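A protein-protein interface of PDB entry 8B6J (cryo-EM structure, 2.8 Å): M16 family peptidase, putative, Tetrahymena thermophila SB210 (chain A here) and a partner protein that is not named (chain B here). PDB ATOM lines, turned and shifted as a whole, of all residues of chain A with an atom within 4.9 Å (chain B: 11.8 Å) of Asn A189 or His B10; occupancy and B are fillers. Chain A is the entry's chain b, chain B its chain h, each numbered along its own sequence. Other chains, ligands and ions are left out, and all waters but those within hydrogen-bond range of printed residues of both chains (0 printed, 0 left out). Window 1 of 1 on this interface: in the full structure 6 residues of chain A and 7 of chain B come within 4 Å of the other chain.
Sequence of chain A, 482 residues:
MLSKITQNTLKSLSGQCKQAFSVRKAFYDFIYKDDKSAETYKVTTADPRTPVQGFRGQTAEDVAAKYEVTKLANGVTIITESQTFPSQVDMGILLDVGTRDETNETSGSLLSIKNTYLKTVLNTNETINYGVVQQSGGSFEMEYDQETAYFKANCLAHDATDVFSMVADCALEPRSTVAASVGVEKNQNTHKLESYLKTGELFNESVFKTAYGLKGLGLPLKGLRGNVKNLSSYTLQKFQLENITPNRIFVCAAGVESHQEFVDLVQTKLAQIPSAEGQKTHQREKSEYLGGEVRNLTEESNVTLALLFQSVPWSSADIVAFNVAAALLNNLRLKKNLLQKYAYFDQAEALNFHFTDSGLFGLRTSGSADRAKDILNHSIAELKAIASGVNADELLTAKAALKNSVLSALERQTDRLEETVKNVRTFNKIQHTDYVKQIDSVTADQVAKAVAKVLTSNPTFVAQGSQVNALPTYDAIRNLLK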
ATOM      1  N   GLU A 185       9.197   9.656  13.132  1.00  0.00           N
ATOM      2  CA  GLU A 185       8.026   9.904  13.970  1.00  0.00           C
ATOM      3  C   GLU A 185       7.653  11.384  13.965  1.00  0.00           C
ATOM      4  O   GLU A 185       6.481  11.751  13.778  1.00  0.00           O
ATOM      5  CB  GLU A 185       8.300   9.420  15.394  1.00  0.00           C
ATOM      6  CG  GLU A 185       7.097   9.481  16.322  1.00  0.00           C
ATOM      7  CD  GLU A 185       6.024   8.477  15.956  1.00  0.00           C
ATOM      8  OE1 GLU A 185       6.229   7.710  14.992  1.00  0.00           O
ATOM      9  OE2 GLU A 185       4.976   8.453  16.635  1.00  0.00           O
ATOM     10  N   LYS A 186       8.647  12.254  14.152  1.00  0.00           N
ATOM     11  CA  LYS A 186       8.373  13.683  14.196  1.00  0.00           C
ATOM     12  C   LYS A 186       7.895  14.207  12.849  1.00  0.00           C
ATOM     13  O   LYS A 186       7.068  15.120  12.804  1.00  0.00           O
ATOM     14  CB  LYS A 186       9.618  14.438  14.656  1.00  0.00           C
ATOM     15  CG  LYS A 186       9.999  14.160  16.098  1.00  0.00           C
ATOM     16  CD  LYS A 186      11.275  14.882  16.487  1.00  0.00           C
ATOM     17  CE  LYS A 186      11.574  14.718  17.967  1.00  0.00           C
ATOM     18  NZ  LYS A 186      12.879  15.323  18.342  1.00  0.00           N
ATOM     19  N   ASN A 187       8.394  13.649  11.746  1.00  0.00           N
ATOM     20  CA  ASN A 187       7.935  14.072  10.430  1.00  0.00           C
ATOM     21  C   ASN A 187       6.490  13.664  10.197  1.00  0.00           C
ATOM     22  O   ASN A 187       5.717  14.419   9.600  1.00  0.00           O
ATOM     23  CB  ASN A 187       8.835  13.485   9.345  1.00  0.00           C
ATOM     24  CG  ASN A 187      10.236  14.045   9.389  1.00  0.00           C
ATOM     25  OD1 ASN A 187      10.681  14.552  10.416  1.00  0.00           O
ATOM     26  ND2 ASN A 187      10.942  13.958   8.270  1.00  0.00           N
ATOM     27  N   GLN A 188       6.106  12.469  10.650  1.00  0.00           N
ATOM     28  CA  GLN A 188       4.700  12.087  10.557  1.00  0.00           C
ATOM     29  C   GLN A 188       3.824  13.046  11.355  1.00  0.00           C
ATOM     30  O   GLN A 188       2.775  13.496  10.871  1.00  0.00           O
ATOM     31  CB  GLN A 188       4.509  10.652  11.041  1.00  0.00           C
ATOM     32  CG  GLN A 188       4.997   9.608  10.056  1.00  0.00           C
ATOM     33  CD  GLN A 188       4.716   8.196  10.519  1.00  0.00           C
ATOM     34  OE1 GLN A 188       4.729   7.909  11.715  1.00  0.00           O
ATOM     35  NE2 GLN A 188       4.451   7.307   9.572  1.00  0.00           N
ATOM     36  N   ASN A 189       4.249  13.386  12.576  1.00  0.00           N
ATOM     37  CA  ASN A 189       3.482  14.343  13.369  1.00  0.00           C
ATOM     38  C   ASN A 189       3.393  15.696  12.671  1.00  0.00           C
ATOM     39  O   ASN A 189       2.329  16.326  12.653  1.00  0.00           O
ATOM     40  CB  ASN A 189       4.104  14.499  14.755  1.00  0.00           C
ATOM     41  CG  ASN A 189       3.823  13.318  15.656  1.00  0.00           C
ATOM     42  OD1 ASN A 189       2.843  12.599  15.466  1.00  0.00           O
ATOM     43  ND2 ASN A 189       4.680  13.113  16.649  1.00  0.00           N
ATOM     44  N   THR A 190       4.505  16.163  12.102  1.00  0.00           N
ATOM     45  CA  THR A 190       4.514  17.455  11.424  1.00  0.00           C
ATOM     46  C   THR A 190       3.587  17.453  10.217  1.00  0.00           C
ATOM     47  O   THR A 190       2.875  18.432   9.973  1.00  0.00           O
ATOM     48  CB  THR A 190       5.938  17.814  10.999  1.00  0.00           C
ATOM     49  OG1 THR A 190       6.752  18.009  12.161  1.00  0.00           O
ATOM     50  CG2 THR A 190       5.946  19.079  10.158  1.00  0.00           C
ATOM     51  N   HIS A 191       3.600  16.374   9.435  1.00  0.00           N
ATOM     52  CA  HIS A 191       2.705  16.288   8.286  1.00  0.00           C
ATOM     53  C   HIS A 191       1.250  16.308   8.729  1.00  0.00           C
ATOM     54  O   HIS A 191       0.418  17.005   8.131  1.00  0.00           O
ATOM     55  CB  HIS A 191       3.002  15.023   7.483  1.00  0.00           C
ATOM     56  CG  HIS A 191       4.315  15.057   6.765  1.00  0.00           C
ATOM     57  ND1 HIS A 191       4.910  13.926   6.250  1.00  0.00           N
ATOM     58  CD2 HIS A 191       5.143  16.085   6.469  1.00  0.00           C
ATOM     59  CE1 HIS A 191       6.051  14.255   5.672  1.00  0.00           C
ATOM     60  NE2 HIS A 191       6.215  15.560   5.789  1.00  0.00           N
ATOM     61  N   LYS A 192       0.921  15.554   9.782  1.00  0.00           N
ATOM     62  CA  LYS A 192      -0.450  15.565  10.278  1.00  0.00           C
ATOM     63  C   LYS A 192      -0.856  16.962  10.726  1.00  0.00           C
ATOM     64  O   LYS A 192      -1.958  17.427  10.413  1.00  0.00           O
ATOM     65  CB  LYS A 192      -0.606  14.572  11.426  1.00  0.00           C
ATOM     66  CG  LYS A 192      -0.596  13.116  10.999  1.00  0.00           C
ATOM     67  CD  LYS A 192      -0.915  12.206  12.170  1.00  0.00           C
ATOM     68  CE  LYS A 192      -0.986  10.752  11.747  1.00  0.00           C
ATOM     69  NZ  LYS A 192      -1.336   9.866  12.890  1.00  0.00           N
ATOM     70  N   LEU A 193       0.023  17.649  11.458  1.00  0.00           N
ATOM     71  CA  LEU A 193      -0.295  18.995  11.924  1.00  0.00           C
ATOM     72  C   LEU A 193      -0.488  19.955  10.756  1.00  0.00           C
ATOM     73  O   LEU A 193      -1.432  20.754  10.747  1.00  0.00           O
ATOM     74  CB  LEU A 193       0.812  19.497  12.849  1.00  0.00           C
ATOM     75  CG  LEU A 193       0.622  20.894  13.436  1.00  0.00           C
ATOM     76  CD1 LEU A 193      -0.600  20.931  14.334  1.00  0.00           C
ATOM     77  CD2 LEU A 193       1.863  21.321  14.198  1.00  0.00           C
ATOM     78  N   VAL B   3      -7.606  25.767  18.014  1.00  0.00           N
ATOM     79  CA  VAL B   3      -7.450  24.456  17.408  1.00  0.00           C
ATOM     80  C   VAL B   3      -7.295  23.411  18.506  1.00  0.00           C
ATOM     81  O   VAL B   3      -6.951  23.717  19.649  1.00  0.00           O
ATOM     82  CB  VAL B   3      -6.243  24.445  16.447  1.00  0.00           C
ATOM     83  CG1 VAL B   3      -6.167  23.136  15.698  1.00  0.00           C
ATOM     84  CG2 VAL B   3      -6.330  25.612  15.476  1.00  0.00           C
ATOM     85  N   THR B   4      -7.560  22.150  18.153  1.00  0.00           N
ATOM     86  CA  THR B   4      -7.468  21.076  19.136  1.00  0.00           C
ATOM     87  C   THR B   4      -6.055  20.956  19.694  1.00  0.00           C
ATOM     88  O   THR B   4      -5.871  20.783  20.905  1.00  0.00           O
ATOM     89  CB  THR B   4      -7.903  19.750  18.510  1.00  0.00           C
ATOM     90  OG1 THR B   4      -7.091  19.470  17.363  1.00  0.00           O
ATOM     91  CG2 THR B   4      -9.365  19.804  18.095  1.00  0.00           C
ATOM     92  N   GLY B   5      -5.049  21.039  18.831  1.00  0.00           N
ATOM     93  CA  GLY B   5      -3.663  20.960  19.235  1.00  0.00           C
ATOM     94  C   GLY B   5      -3.029  22.284  19.592  1.00  0.00           C
ATOM     95  O   GLY B   5      -1.821  22.324  19.848  1.00  0.00           O
ATOM     96  N   ALA B   6      -3.803  23.368  19.616  1.00  0.00           N
ATOM     97  CA  ALA B   6      -3.353  24.732  19.896  1.00  0.00           C
ATOM     98  C   ALA B   6      -2.647  25.353  18.700  1.00  0.00           C
ATOM     99  O   ALA B   6      -2.101  26.457  18.824  1.00  0.00           O
ATOM    100  CB  ALA B   6      -2.424  24.806  21.111  1.00  0.00           C
ATOM    101  N   GLY B   7      -2.635  24.686  17.548  1.00  0.00           N
ATOM    102  CA  GLY B   7      -2.092  25.259  16.336  1.00  0.00           C
ATOM    103  C   GLY B   7      -0.598  25.114  16.150  1.00  0.00           C
ATOM    104  O   GLY B   7      -0.064  25.648  15.170  1.00  0.00           O
ATOM    105  N   LEU B   8       0.101  24.422  17.052  1.00  0.00           N
ATOM    106  CA  LEU B   8       1.537  24.236  16.899  1.00  0.00           C
ATOM    107  C   LEU B   8       2.020  22.828  17.219  1.00  0.00           C
ATOM    108  O   LEU B   8       3.228  22.583  17.135  1.00  0.00           O
ATOM    109  CB  LEU B   8       2.300  25.249  17.771  1.00  0.00           C
ATOM    110  CG  LEU B   8       1.805  25.474  19.203  1.00  0.00           C
ATOM    111  CD1 LEU B   8       1.905  24.217  20.055  1.00  0.00           C
ATOM    112  CD2 LEU B   8       2.574  26.620  19.847  1.00  0.00           C
ATOM    113  N   THR B   9       1.136  21.900  17.577  1.00  0.00           N
ATOM    114  CA  THR B   9       1.534  20.517  17.798  1.00  0.00           C
ATOM    115  C   THR B   9       0.366  19.601  17.471  1.00  0.00           C
ATOM    116  O   THR B   9      -0.795  20.018  17.454  1.00  0.00           O
ATOM    117  CB  THR B   9       2.000  20.270  19.238  1.00  0.00           C
ATOM    118  OG1 THR B   9       1.153  20.980  20.150  1.00  0.00           O
ATOM    119  CG2 THR B   9       3.446  20.708  19.421  1.00  0.00           C
ATOM    120  N   HIS B  10       0.694  18.339  17.211  1.00  0.00           N
ATOM    121  CA  HIS B  10      -0.289  17.314  16.894  1.00  0.00           C
ATOM    122  C   HIS B  10      -0.515  16.442  18.120  1.00  0.00           C
ATOM    123  O   HIS B  10       0.444  16.020  18.774  1.00  0.00           O
ATOM    124  CB  HIS B  10       0.178  16.461  15.716  1.00  0.00           C
ATOM    125  CG  HIS B  10      -0.772  15.365  15.352  1.00  0.00           C
ATOM    126  ND1 HIS B  10      -2.027  15.610  14.838  1.00  0.00           N
ATOM    127  CD2 HIS B  10      -0.653  14.019  15.428  1.00  0.00           C
ATOM    128  CE1 HIS B  10      -2.640  14.462  14.613  1.00  0.00           C
ATOM    129  NE2 HIS B  10      -1.828  13.480  14.963  1.00  0.00           N
ATOM    130  N   VAL B  11      -1.783  16.179  18.430  1.00  0.00           N
ATOM    131  CA  VAL B  11      -2.172  15.404  19.601  1.00  0.00           C
ATOM    132  C   VAL B  11      -2.796  14.098  19.132  1.00  0.00           C
ATOM    133  O   VAL B  11      -3.738  14.105  18.330  1.00  0.00           O
ATOM    134  CB  VAL B  11      -3.151  16.188  20.491  1.00  0.00           C
ATOM    135  CG1 VAL B  11      -3.573  15.350  21.686  1.00  0.00           C
ATOM    136  CG2 VAL B  11      -2.522  17.494  20.947  1.00  0.00           C
ATOM    137  N   LYS B  12      -2.273  12.980  19.631  1.00  0.00           N
ATOM    138  CA  LYS B  12      -2.842  11.664  19.352  1.00  0.00           C
ATOM    139  C   LYS B  12      -4.001  11.458  20.315  1.00  0.00           C
ATOM    140  O   LYS B  12      -3.830  11.009  21.449  1.00  0.00           O
ATOM    141  CB  LYS B  12      -1.787  10.573  19.493  1.00  0.00           C
ATOM    142  CG  LYS B  12      -0.665  10.672  18.475  1.00  0.00           C
ATOM    143  CD  LYS B  12       0.323   9.527  18.619  1.00  0.00           C
ATOM    144  CE  LYS B  12       1.431   9.618  17.581  1.00  0.00           C
ATOM    145  NZ  LYS B  12       2.414   8.508  17.711  1.00  0.00           N
ATOM    146  N   ASP B  13      -5.199  11.788  19.849  1.00  0.00           N
ATOM    147  CA  ASP B  13      -6.386  11.852  20.682  1.00  0.00           C
ATOM    148  C   ASP B  13      -7.398  10.807  20.228  1.00  0.00           C
ATOM    149  O   ASP B  13      -7.399  10.375  19.073  1.00  0.00           O
ATOM    150  CB  ASP B  13      -7.011  13.249  20.624  1.00  0.00           C
ATOM    151  CG  ASP B  13      -7.735  13.614  21.894  1.00  0.00           C
ATOM    152  OD1 ASP B  13      -8.204  12.691  22.590  1.00  0.00           O
ATOM    153  OD2 ASP B  13      -7.829  14.821  22.196  1.00  0.00           O
ATOM    154  N   PHE B  14      -8.262  10.402  21.156  1.00  0.00           N
ATOM    155  CA  PHE B  14      -9.261   9.382  20.859  1.00  0.00           C
ATOM    156  C   PHE B  14     -10.341   9.415  21.927  1.00  0.00           C
ATOM    157  O   PHE B  14     -10.035   9.378  23.121  1.00  0.00           O
ATOM    158  CB  PHE B  14      -8.613   7.997  20.792  1.00  0.00           C
ATOM    159  CG  PHE B  14      -9.575   6.895  20.468  1.00  0.00           C
ATOM    160  CD1 PHE B  14      -9.994   6.685  19.168  1.00  0.00           C
ATOM    161  CD2 PHE B  14     -10.054   6.065  21.463  1.00  0.00           C
ATOM    162  CE1 PHE B  14     -10.878   5.671  18.868  1.00  0.00           C
ATOM    163  CE2 PHE B  14     -10.936   5.053  21.169  1.00  0.00           C
ATOM    164  CZ  PHE B  14     -11.348   4.853  19.870  1.00  0.00           C
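OG1 of Thr B9 is in hydrogen-bond range of O of Gly B5, at 3.3 Å.
His B10 touches Asn A189.
OD1 of Asn A189 touches CE of Lys B12, at 3.9 Å.
His B10 touches Lys A192 (NE2 to CD, 3.2 Å).
Leu A193 touches Leu B8 (CD2 to C, 3.4 Å).
CD1 of Leu A193 touches O of Thr B9 (3.3 Å).
Of the 12 printed residues of chain B, 4 touch a printed residue of chain A.
Hydrophobic or aromatic side chains of chain B that line the printed part of chain A: His B10.
Among the printed residues, 6 pairs touch across the chains.
Asn A189 touches just these residues of chain B: His B10 (3.7 Å) and Lys B12 (3.9 Å).
Of chain A, only Asn A189 and Lys A192 come within 4 Å of His B10.
No residue of chain B comes within 4 Å of Gln A188.
No residue of chain B comes within 4 Å of His A191.
Of the printed residues of chain A, Leu B8 touches Leu A193.
Of the printed residues of chain A, Thr B9 touches Leu A193.
Printed residues of chain A within 4 Å of Lys B12: Glu A185 (2.8 Å) and Asn A189 (3.9 Å).
Thr B4 touches none of the printed residues of chain A.
Ala B6 touches none of the printed residues of chain A.
The nearest residue of chain B that does not touch Asn A189 is Thr B9 (6.1 Å).
The side-chain carboxylate of Glu A185 lies within salt-bridge range of the side-chain amino group of Lys B12, at 2.8 Å.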
